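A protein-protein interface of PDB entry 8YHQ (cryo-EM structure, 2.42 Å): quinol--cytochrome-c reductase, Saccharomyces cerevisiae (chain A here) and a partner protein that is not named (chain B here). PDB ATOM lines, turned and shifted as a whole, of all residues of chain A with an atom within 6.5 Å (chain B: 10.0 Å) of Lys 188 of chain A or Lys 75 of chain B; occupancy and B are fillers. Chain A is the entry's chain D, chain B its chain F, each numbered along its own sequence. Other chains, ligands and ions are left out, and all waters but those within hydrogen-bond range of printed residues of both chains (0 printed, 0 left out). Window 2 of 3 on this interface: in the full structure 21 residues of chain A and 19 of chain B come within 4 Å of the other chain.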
ATOM      1  N   TRP A  15       5.808   4.220   9.539  1.00  0.00           N
ATOM      2  CA  TRP A  15       4.594   3.784   8.869  1.00  0.00           C
ATOM      3  C   TRP A  15       3.752   4.974   8.438  1.00  0.00           C
ATOM      4  O   TRP A  15       3.645   5.975   9.150  1.00  0.00           O
ATOM      5  CB  TRP A  15       3.790   2.870   9.781  1.00  0.00           C
ATOM      6  CG  TRP A  15       4.501   1.599  10.117  1.00  0.00           C
ATOM      7  CD1 TRP A  15       5.306   1.373  11.186  1.00  0.00           C
ATOM      8  CD2 TRP A  15       4.475   0.378   9.372  1.00  0.00           C
ATOM      9  NE1 TRP A  15       5.784   0.092  11.158  1.00  0.00           N
ATOM     10  CE2 TRP A  15       5.289  -0.541  10.052  1.00  0.00           C
ATOM     11  CE3 TRP A  15       3.841  -0.027   8.196  1.00  0.00           C
ATOM     12  CZ2 TRP A  15       5.483  -1.836   9.598  1.00  0.00           C
ATOM     13  CZ3 TRP A  15       4.039  -1.305   7.750  1.00  0.00           C
ATOM     14  CH2 TRP A  15       4.852  -2.197   8.448  1.00  0.00           C
ATOM     15  N   SER A  16       3.154   4.855   7.256  1.00  0.00           N
ATOM     16  CA  SER A  16       2.408   5.933   6.627  1.00  0.00           C
ATOM     17  C   SER A  16       1.068   6.227   7.289  1.00  0.00           C
ATOM     18  O   SER A  16       0.471   7.265   6.984  1.00  0.00           O
ATOM     19  CB  SER A  16       2.178   5.597   5.157  1.00  0.00           C
ATOM     20  OG  SER A  16       1.364   6.560   4.535  1.00  0.00           O
ATOM     21  N   ASP A  25      -2.935   3.443   3.664  1.00  0.00           N
ATOM     22  CA  ASP A  25      -2.642   3.398   2.235  1.00  0.00           C
ATOM     23  C   ASP A  25      -3.350   2.194   1.628  1.00  0.00           C
ATOM     24  O   ASP A  25      -2.975   1.048   1.888  1.00  0.00           O
ATOM     25  CB  ASP A  25      -1.136   3.331   2.017  1.00  0.00           C
ATOM     26  CG  ASP A  25      -0.746   3.408   0.553  1.00  0.00           C
ATOM     27  OD1 ASP A  25      -1.625   3.640  -0.302  1.00  0.00           O
ATOM     28  OD2 ASP A  25       0.452   3.235   0.255  1.00  0.00           O
ATOM     29  N   ALA A  27      -3.636   1.067  -1.486  1.00  0.00           N
ATOM     30  CA  ALA A  27      -2.959   0.259  -2.488  1.00  0.00           C
ATOM     31  C   ALA A  27      -2.058  -0.790  -1.854  1.00  0.00           C
ATOM     32  O   ALA A  27      -1.819  -1.842  -2.454  1.00  0.00           O
ATOM     33  CB  ALA A  27      -2.147   1.151  -3.417  1.00  0.00           C
ATOM     34  N   SER A  28      -1.547  -0.517  -0.656  1.00  0.00           N
ATOM     35  CA  SER A  28      -0.779  -1.503   0.086  1.00  0.00           C
ATOM     36  C   SER A  28      -1.670  -2.572   0.710  1.00  0.00           C
ATOM     37  O   SER A  28      -1.230  -3.713   0.879  1.00  0.00           O
ATOM     38  CB  SER A  28       0.050  -0.798   1.153  1.00  0.00           C
ATOM     39  OG  SER A  28       0.884  -1.693   1.848  1.00  0.00           O
ATOM     40  N   ARG A  31      -2.456  -4.984  -2.265  1.00  0.00           N
ATOM     41  CA  ARG A  31      -1.305  -5.842  -2.502  1.00  0.00           C
ATOM     42  C   ARG A  31      -1.076  -6.816  -1.354  1.00  0.00           C
ATOM     43  O   ARG A  31      -0.596  -7.931  -1.579  1.00  0.00           O
ATOM     44  CB  ARG A  31      -0.060  -4.987  -2.725  1.00  0.00           C
ATOM     45  CG  ARG A  31       0.113  -4.480  -4.135  1.00  0.00           C
ATOM     46  CD  ARG A  31       1.430  -3.761  -4.321  1.00  0.00           C
ATOM     47  NE  ARG A  31       1.325  -2.329  -4.029  1.00  0.00           N
ATOM     48  CZ  ARG A  31       2.067  -1.642  -3.163  1.00  0.00           C
ATOM     49  NH1 ARG A  31       1.844  -0.353  -3.019  1.00  0.00           N
ATOM     50  NH2 ARG A  31       3.023  -2.200  -2.437  1.00  0.00           N
ATOM     51  N   PHE A 131       6.513  -7.034  11.290  1.00  0.00           N
ATOM     52  CA  PHE A 131       7.469  -6.819  10.209  1.00  0.00           C
ATOM     53  C   PHE A 131       8.847  -7.359  10.570  1.00  0.00           C
ATOM     54  O   PHE A 131       9.487  -8.045   9.764  1.00  0.00           O
ATOM     55  CB  PHE A 131       7.544  -5.327   9.884  1.00  0.00           C
ATOM     56  CG  PHE A 131       8.442  -4.995   8.734  1.00  0.00           C
ATOM     57  CD1 PHE A 131       7.953  -4.963   7.451  1.00  0.00           C
ATOM     58  CD2 PHE A 131       9.773  -4.700   8.937  1.00  0.00           C
ATOM     59  CE1 PHE A 131       8.771  -4.660   6.400  1.00  0.00           C
ATOM     60  CE2 PHE A 131      10.592  -4.402   7.884  1.00  0.00           C
ATOM     61  CZ  PHE A 131      10.089  -4.380   6.617  1.00  0.00           C
ATOM     62  N   ASP A 177       0.169  -4.482 -10.296  1.00  0.00           N
ATOM     63  CA  ASP A 177       0.469  -3.085 -10.569  1.00  0.00           C
ATOM     64  C   ASP A 177       1.942  -2.841 -10.881  1.00  0.00           C
ATOM     65  O   ASP A 177       2.347  -1.685 -11.033  1.00  0.00           O
ATOM     66  CB  ASP A 177       0.024  -2.219  -9.388  1.00  0.00           C
ATOM     67  CG  ASP A 177       0.783  -2.524  -8.110  1.00  0.00           C
ATOM     68  OD1 ASP A 177       1.456  -3.572  -8.039  1.00  0.00           O
ATOM     69  OD2 ASP A 177       0.708  -1.708  -7.172  1.00  0.00           O
ATOM     70  N   THR A 179       4.815  -3.600  -9.086  1.00  0.00           N
ATOM     71  CA  THR A 179       5.737  -3.273  -8.007  1.00  0.00           C
ATOM     72  C   THR A 179       6.801  -4.365  -7.877  1.00  0.00           C
ATOM     73  O   THR A 179       6.481  -5.550  -7.992  1.00  0.00           O
ATOM     74  CB  THR A 179       4.988  -3.135  -6.686  1.00  0.00           C
ATOM     75  OG1 THR A 179       3.857  -2.275  -6.860  1.00  0.00           O
ATOM     76  CG2 THR A 179       5.882  -2.567  -5.608  1.00  0.00           C
ATOM     77  N   PRO A 180       8.079  -4.048  -7.655  1.00  0.00           N
ATOM     78  CA  PRO A 180       9.053  -5.118  -7.391  1.00  0.00           C
ATOM     79  C   PRO A 180       8.749  -5.831  -6.084  1.00  0.00           C
ATOM     80  O   PRO A 180       8.696  -5.216  -5.018  1.00  0.00           O
ATOM     81  CB  PRO A 180      10.391  -4.373  -7.337  1.00  0.00           C
ATOM     82  CG  PRO A 180      10.163  -3.122  -8.058  1.00  0.00           C
ATOM     83  CD  PRO A 180       8.751  -2.747  -7.803  1.00  0.00           C
ATOM     84  N   THR A 183      11.498  -9.035  -0.635  1.00  0.00           N
ATOM     85  CA  THR A 183      11.103  -9.592   0.654  1.00  0.00           C
ATOM     86  C   THR A 183      10.479  -8.530   1.553  1.00  0.00           C
ATOM     87  O   THR A 183       9.425  -8.756   2.159  1.00  0.00           O
ATOM     88  CB  THR A 183      12.319 -10.226   1.325  1.00  0.00           C
ATOM     89  OG1 THR A 183      12.834 -11.270   0.494  1.00  0.00           O
ATOM     90  CG2 THR A 183      11.963 -10.799   2.677  1.00  0.00           C
ATOM     91  N   SER A 184      11.122  -7.366   1.660  1.00  0.00           N
ATOM     92  CA  SER A 184      10.614  -6.315   2.534  1.00  0.00           C
ATOM     93  C   SER A 184       9.309  -5.736   2.010  1.00  0.00           C
ATOM     94  O   SER A 184       8.427  -5.369   2.792  1.00  0.00           O
ATOM     95  CB  SER A 184      11.652  -5.210   2.682  1.00  0.00           C
ATOM     96  OG  SER A 184      12.828  -5.698   3.297  1.00  0.00           O
ATOM     97  N   GLN A 185       9.178  -5.633   0.688  1.00  0.00           N
ATOM     98  CA  GLN A 185       7.980  -5.054   0.097  1.00  0.00           C
ATOM     99  C   GLN A 185       6.744  -5.876   0.440  1.00  0.00           C
ATOM    100  O   GLN A 185       5.697  -5.326   0.800  1.00  0.00           O
ATOM    101  CB  GLN A 185       8.169  -4.944  -1.414  1.00  0.00           C
ATOM    102  CG  GLN A 185       7.077  -4.212  -2.163  1.00  0.00           C
ATOM    103  CD  GLN A 185       7.054  -2.743  -1.851  1.00  0.00           C
ATOM    104  OE1 GLN A 185       8.063  -2.056  -1.974  1.00  0.00           O
ATOM    105  NE2 GLN A 185       5.898  -2.247  -1.444  1.00  0.00           N
ATOM    106  N   MET A 186       6.846  -7.201   0.339  1.00  0.00           N
ATOM    107  CA  MET A 186       5.707  -8.055   0.646  1.00  0.00           C
ATOM    108  C   MET A 186       5.413  -8.070   2.142  1.00  0.00           C
ATOM    109  O   MET A 186       4.249  -8.136   2.550  1.00  0.00           O
ATOM    110  CB  MET A 186       5.969  -9.468   0.136  1.00  0.00           C
ATOM    111  CG  MET A 186       6.143  -9.562  -1.359  1.00  0.00           C
ATOM    112  SD  MET A 186       6.219 -11.257  -1.957  1.00  0.00           S
ATOM    113  CE  MET A 186       7.877 -11.712  -1.474  1.00  0.00           C
ATOM    114  N   ALA A 187       6.456  -8.023   2.973  1.00  0.00           N
ATOM    115  CA  ALA A 187       6.265  -7.984   4.419  1.00  0.00           C
ATOM    116  C   ALA A 187       5.520  -6.725   4.845  1.00  0.00           C
ATOM    117  O   ALA A 187       4.654  -6.770   5.726  1.00  0.00           O
ATOM    118  CB  ALA A 187       7.615  -8.073   5.126  1.00  0.00           C
ATOM    119  N   LYS A 188       5.852  -5.588   4.233  1.00  0.00           N
ATOM    120  CA  LYS A 188       5.184  -4.335   4.564  1.00  0.00           C
ATOM    121  C   LYS A 188       3.712  -4.369   4.181  1.00  0.00           C
ATOM    122  O   LYS A 188       2.857  -3.901   4.940  1.00  0.00           O
ATOM    123  CB  LYS A 188       5.900  -3.174   3.875  1.00  0.00           C
ATOM    124  CG  LYS A 188       5.132  -1.887   3.802  1.00  0.00           C
ATOM    125  CD  LYS A 188       6.010  -0.783   3.310  1.00  0.00           C
ATOM    126  CE  LYS A 188       5.219   0.469   3.047  1.00  0.00           C
ATOM    127  NZ  LYS A 188       4.358   0.360   1.858  1.00  0.00           N
ATOM    128  N   ASP A 189       3.394  -4.898   3.001  1.00  0.00           N
ATOM    129  CA  ASP A 189       2.009  -4.925   2.554  1.00  0.00           C
ATOM    130  C   ASP A 189       1.188  -5.928   3.358  1.00  0.00           C
ATOM    131  O   ASP A 189      -0.008  -5.719   3.585  1.00  0.00           O
ATOM    132  CB  ASP A 189       1.956  -5.236   1.057  1.00  0.00           C
ATOM    133  CG  ASP A 189       2.636  -4.178   0.214  1.00  0.00           C
ATOM    134  OD1 ASP A 189       2.682  -3.006   0.633  1.00  0.00           O
ATOM    135  OD2 ASP A 189       3.128  -4.520  -0.879  1.00  0.00           O
ATOM    136  N   VAL A 190       1.816  -7.018   3.801  1.00  0.00           N
ATOM    137  CA  VAL A 190       1.134  -8.000   4.641  1.00  0.00           C
ATOM    138  C   VAL A 190       0.723  -7.374   5.968  1.00  0.00           C
ATOM    139  O   VAL A 190      -0.413  -7.537   6.426  1.00  0.00           O
ATOM    140  CB  VAL A 190       2.036  -9.231   4.845  1.00  0.00           C
ATOM    141  CG1 VAL A 190       1.568 -10.108   5.963  1.00  0.00           C
ATOM    142  CG2 VAL A 190       2.015 -10.038   3.631  1.00  0.00           C
ATOM    143  N   THR A 191       1.651  -6.665   6.610  1.00  0.00           N
ATOM    144  CA  THR A 191       1.371  -6.081   7.916  1.00  0.00           C
ATOM    145  C   THR A 191       0.313  -4.989   7.822  1.00  0.00           C
ATOM    146  O   THR A 191      -0.501  -4.829   8.736  1.00  0.00           O
ATOM    147  CB  THR A 191       2.662  -5.538   8.525  1.00  0.00           C
ATOM    148  OG1 THR A 191       3.653  -6.568   8.560  1.00  0.00           O
ATOM    149  CG2 THR A 191       2.419  -5.050   9.911  1.00  0.00           C
ATOM    150  N   THR A 192       0.309  -4.228   6.727  1.00  0.00           N
ATOM    151  CA  THR A 192      -0.696  -3.190   6.537  1.00  0.00           C
ATOM    152  C   THR A 192      -2.085  -3.788   6.357  1.00  0.00           C
ATOM    153  O   THR A 192      -3.066  -3.275   6.904  1.00  0.00           O
ATOM    154  CB  THR A 192      -0.313  -2.325   5.340  1.00  0.00           C
ATOM    155  OG1 THR A 192       1.054  -1.931   5.465  1.00  0.00           O
ATOM    156  CG2 THR A 192      -1.169  -1.090   5.252  1.00  0.00           C
ATOM    157  N   PHE A 193      -2.192  -4.859   5.572  1.00  0.00           N
ATOM    158  CA  PHE A 193      -3.460  -5.563   5.433  1.00  0.00           C
ATOM    159  C   PHE A 193      -3.936  -6.115   6.770  1.00  0.00           C
ATOM    160  O   PHE A 193      -5.126  -6.041   7.091  1.00  0.00           O
ATOM    161  CB  PHE A 193      -3.302  -6.676   4.398  1.00  0.00           C
ATOM    162  CG  PHE A 193      -4.420  -7.665   4.382  1.00  0.00           C
ATOM    163  CD1 PHE A 193      -5.657  -7.320   3.897  1.00  0.00           C
ATOM    164  CD2 PHE A 193      -4.228  -8.950   4.836  1.00  0.00           C
ATOM    165  CE1 PHE A 193      -6.676  -8.222   3.878  1.00  0.00           C
ATOM    166  CE2 PHE A 193      -5.246  -9.852   4.818  1.00  0.00           C
ATOM    167  CZ  PHE A 193      -6.473  -9.489   4.336  1.00  0.00           C
ATOM    168  N   ASP B   4      16.624  -6.925  -1.869  1.00  0.00           N
ATOM    169  CA  ASP B   4      15.818  -6.411  -0.776  1.00  0.00           C
ATOM    170  C   ASP B   4      16.523  -5.219  -0.136  1.00  0.00           C
ATOM    171  O   ASP B   4      17.678  -5.303   0.281  1.00  0.00           O
ATOM    172  CB  ASP B   4      15.582  -7.515   0.254  1.00  0.00           C
ATOM    173  CG  ASP B   4      14.531  -7.155   1.265  1.00  0.00           C
ATOM    174  OD1 ASP B   4      13.720  -6.262   0.971  1.00  0.00           O
ATOM    175  OD2 ASP B   4      14.523  -7.757   2.361  1.00  0.00           O
ATOM    176  N   GLN B   5      15.802  -4.104  -0.038  1.00  0.00           N
ATOM    177  CA  GLN B   5      16.441  -2.844   0.328  1.00  0.00           C
ATOM    178  C   GLN B   5      16.960  -2.864   1.758  1.00  0.00           C
ATOM    179  O   GLN B   5      17.978  -2.235   2.059  1.00  0.00           O
ATOM    180  CB  GLN B   5      15.468  -1.683   0.140  1.00  0.00           C
ATOM    181  CG  GLN B   5      15.038  -1.416  -1.287  1.00  0.00           C
ATOM    182  CD  GLN B   5      13.874  -2.268  -1.726  1.00  0.00           C
ATOM    183  OE1 GLN B   5      13.366  -3.082  -0.961  1.00  0.00           O
ATOM    184  NE2 GLN B   5      13.437  -2.080  -2.957  1.00  0.00           N
ATOM    185  N   LEU B   6      16.276  -3.575   2.654  1.00  0.00           N
ATOM    186  CA  LEU B   6      16.759  -3.697   4.024  1.00  0.00           C
ATOM    187  C   LEU B   6      18.077  -4.456   4.067  1.00  0.00           C
ATOM    188  O   LEU B   6      18.992  -4.082   4.804  1.00  0.00           O
ATOM    189  CB  LEU B   6      15.697  -4.386   4.881  1.00  0.00           C
ATOM    190  CG  LEU B   6      16.009  -4.742   6.335  1.00  0.00           C
ATOM    191  CD1 LEU B   6      16.575  -3.576   7.118  1.00  0.00           C
ATOM    192  CD2 LEU B   6      14.746  -5.248   6.999  1.00  0.00           C
ATOM    193  N   LEU B  70      14.430   3.092   5.856  1.00  0.00           N
ATOM    194  CA  LEU B  70      14.080   2.043   4.906  1.00  0.00           C
ATOM    195  C   LEU B  70      12.835   2.402   4.106  1.00  0.00           C
ATOM    196  O   LEU B  70      12.852   2.387   2.871  1.00  0.00           O
ATOM    197  CB  LEU B  70      13.872   0.724   5.648  1.00  0.00           C
ATOM    198  CG  LEU B  70      13.471  -0.493   4.821  1.00  0.00           C
ATOM    199  CD1 LEU B  70      14.584  -0.865   3.867  1.00  0.00           C
ATOM    200  CD2 LEU B  70      13.139  -1.629   5.723  1.00  0.00           C
ATOM    201  N   PHE B  71      11.742   2.719   4.797  1.00  0.00           N
ATOM    202  CA  PHE B  71      10.452   2.910   4.142  1.00  0.00           C
ATOM    203  C   PHE B  71      10.449   4.086   3.173  1.00  0.00           C
ATOM    204  O   PHE B  71       9.530   4.187   2.353  1.00  0.00           O
ATOM    205  CB  PHE B  71       9.358   3.085   5.201  1.00  0.00           C
ATOM    206  CG  PHE B  71       8.849   1.795   5.794  1.00  0.00           C
ATOM    207  CD1 PHE B  71       9.659   0.678   5.906  1.00  0.00           C
ATOM    208  CD2 PHE B  71       7.550   1.708   6.247  1.00  0.00           C
ATOM    209  CE1 PHE B  71       9.184  -0.483   6.442  1.00  0.00           C
ATOM    210  CE2 PHE B  71       7.076   0.546   6.787  1.00  0.00           C
ATOM    211  CZ  PHE B  71       7.891  -0.551   6.888  1.00  0.00           C
ATOM    212  N   ASP B  72      11.446   4.970   3.242  1.00  0.00           N
ATOM    213  CA  ASP B  72      11.628   5.986   2.213  1.00  0.00           C
ATOM    214  C   ASP B  72      11.857   5.380   0.836  1.00  0.00           C
ATOM    215  O   ASP B  72      11.533   6.020  -0.169  1.00  0.00           O
ATOM    216  CB  ASP B  72      12.819   6.885   2.564  1.00  0.00           C
ATOM    217  CG  ASP B  72      12.432   8.106   3.390  1.00  0.00           C
ATOM    218  OD1 ASP B  72      11.235   8.316   3.677  1.00  0.00           O
ATOM    219  OD2 ASP B  72      13.348   8.869   3.761  1.00  0.00           O
ATOM    220  N   LYS B  73      12.401   4.164   0.766  1.00  0.00           N
ATOM    221  CA  LYS B  73      12.744   3.525  -0.495  1.00  0.00           C
ATOM    222  C   LYS B  73      11.755   2.459  -0.933  1.00  0.00           C
ATOM    223  O   LYS B  73      11.634   2.208  -2.133  1.00  0.00           O
ATOM    224  CB  LYS B  73      14.135   2.896  -0.400  1.00  0.00           C
ATOM    225  CG  LYS B  73      15.166   3.827   0.212  1.00  0.00           C
ATOM    226  CD  LYS B  73      16.573   3.494  -0.218  1.00  0.00           C
ATOM    227  CE  LYS B  73      17.059   2.229   0.443  1.00  0.00           C
ATOM    228  NZ  LYS B  73      18.408   1.857  -0.045  1.00  0.00           N
ATOM    229  N   LEU B  74      11.055   1.822  -0.002  1.00  0.00           N
ATOM    230  CA  LEU B  74      10.022   0.869  -0.372  1.00  0.00           C
ATOM    231  C   LEU B  74       8.779   1.608  -0.838  1.00  0.00           C
ATOM    232  O   LEU B  74       8.392   2.631  -0.268  1.00  0.00           O
ATOM    233  CB  LEU B  74       9.678  -0.037   0.806  1.00  0.00           C
ATOM    234  CG  LEU B  74      10.832  -0.752   1.500  1.00  0.00           C
ATOM    235  CD1 LEU B  74      10.334  -1.369   2.778  1.00  0.00           C
ATOM    236  CD2 LEU B  74      11.457  -1.800   0.601  1.00  0.00           C
ATOM    237  N   LYS B  75       8.159   1.087  -1.886  1.00  0.00           N
ATOM    238  CA  LYS B  75       6.942   1.670  -2.426  1.00  0.00           C
ATOM    239  C   LYS B  75       5.796   1.524  -1.431  1.00  0.00           C
ATOM    240  O   LYS B  75       4.766   2.185  -1.538  1.00  0.00           O
ATOM    241  CB  LYS B  75       6.584   1.006  -3.758  1.00  0.00           C
ATOM    242  CG  LYS B  75       5.754   1.848  -4.698  1.00  0.00           C
ATOM    243  CD  LYS B  75       4.309   1.412  -4.685  1.00  0.00           C
ATOM    244  CE  LYS B  75       3.403   2.456  -5.323  1.00  0.00           C
ATOM    245  NZ  LYS B  75       1.952   2.135  -5.189  1.00  0.00           N
ATOM    246  OXT LYS B  75       5.875   0.737  -0.490  1.00  0.00           O
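Hydrophobic or aromatic side chains of chain B within 4 Å of the printed part of chain A: Leu 6, Phe 71 and Leu 74. Of the 21 printed residues of chain A, 6 touch a printed residue of chain B. Printed residues of chain A that touch a printed residue of chain B: Trp 15, Arg 31, Thr 183, Ser 184, Gln 185 and Lys 188.
Among the printed residues, merely in contact across the chains: Thr 183 of chain A with Asp 4 of chain B, Ser 184 of chain A with Leu 6 of chain B, Trp 15 of chain A with Phe 71 of chain B, Gln 185 of chain A with Leu 74 of chain B, Lys 188 of chain A with Phe 71 of chain B and Ser 184 of chain A with Leu 74 of chain B.
The side-chain carboxylate of Asp 177 of chain A is in salt-bridge range of the guanidinium group of Arg 31 of chain A (3.3 Å). The guanidinium group (NH2) of Arg 31 of chain A sits close to the side-chain amide nitrogen (NE2) of Gln 185 of chain A (3.0 Å). NH2 of Arg 31 of chain A lies within salt-bridge range of OD2 of Asp 189 of chain A, at 2.8 Å. NZ of Lys 188 of chain A lies within salt-bridge range of OD1 of Asp 189 of chain A, 3.95 Å away. OG1 of Thr 192 of chain A lies within hydrogen-bond range of O of Lys 188 of chain A (2.7 Å).
The side-chain carboxylate (OD1) of Asp 4 of chain B is in hydrogen-bond range of the side-chain hydroxyl (OG) of Ser 184 of chain A. NE2 of Gln 185 of chain A is in hydrogen-bond range of OXT of Lys 75 of chain B (3.1 Å). The side-chain amino group (NZ) of Lys 188 of chain A lies within salt-bridge range of the chain-end carboxylate (OXT) of Lys 75 of chain B, at 2.8 Å. NZ of Lys 75 of chain B sits close to NH1 of Arg 31 of chain A, 3.3 Å away.
Of chain B, only Phe 71 and Lys 75 come within 4 Å of Lys 188 of chain A. No residue of chain B comes within 4 Å of Asp 189 of chain A. No residue of chain B comes within 4 Å of Thr 191 of chain A. Printed residues of chain A within 4 Å of Leu 74 of chain B: Ser 184 (3.9996 Å) and Gln 185 (3.8 Å). Of the printed residues of chain B, Arg 31 of chain A touches Lys 75 (3.3 Å). Printed residues of chain B within 4 Å of Gln 185 of chain A: Leu 74 and Lys 75. Pro 180 of chain A touches none of the printed residues of chain B. Leu 70 of chain B touches none of the printed residues of chain A. The nearest residue of chain A that does not touch Lys 75 of chain B is Thr 179 of chain A (4.1 Å).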
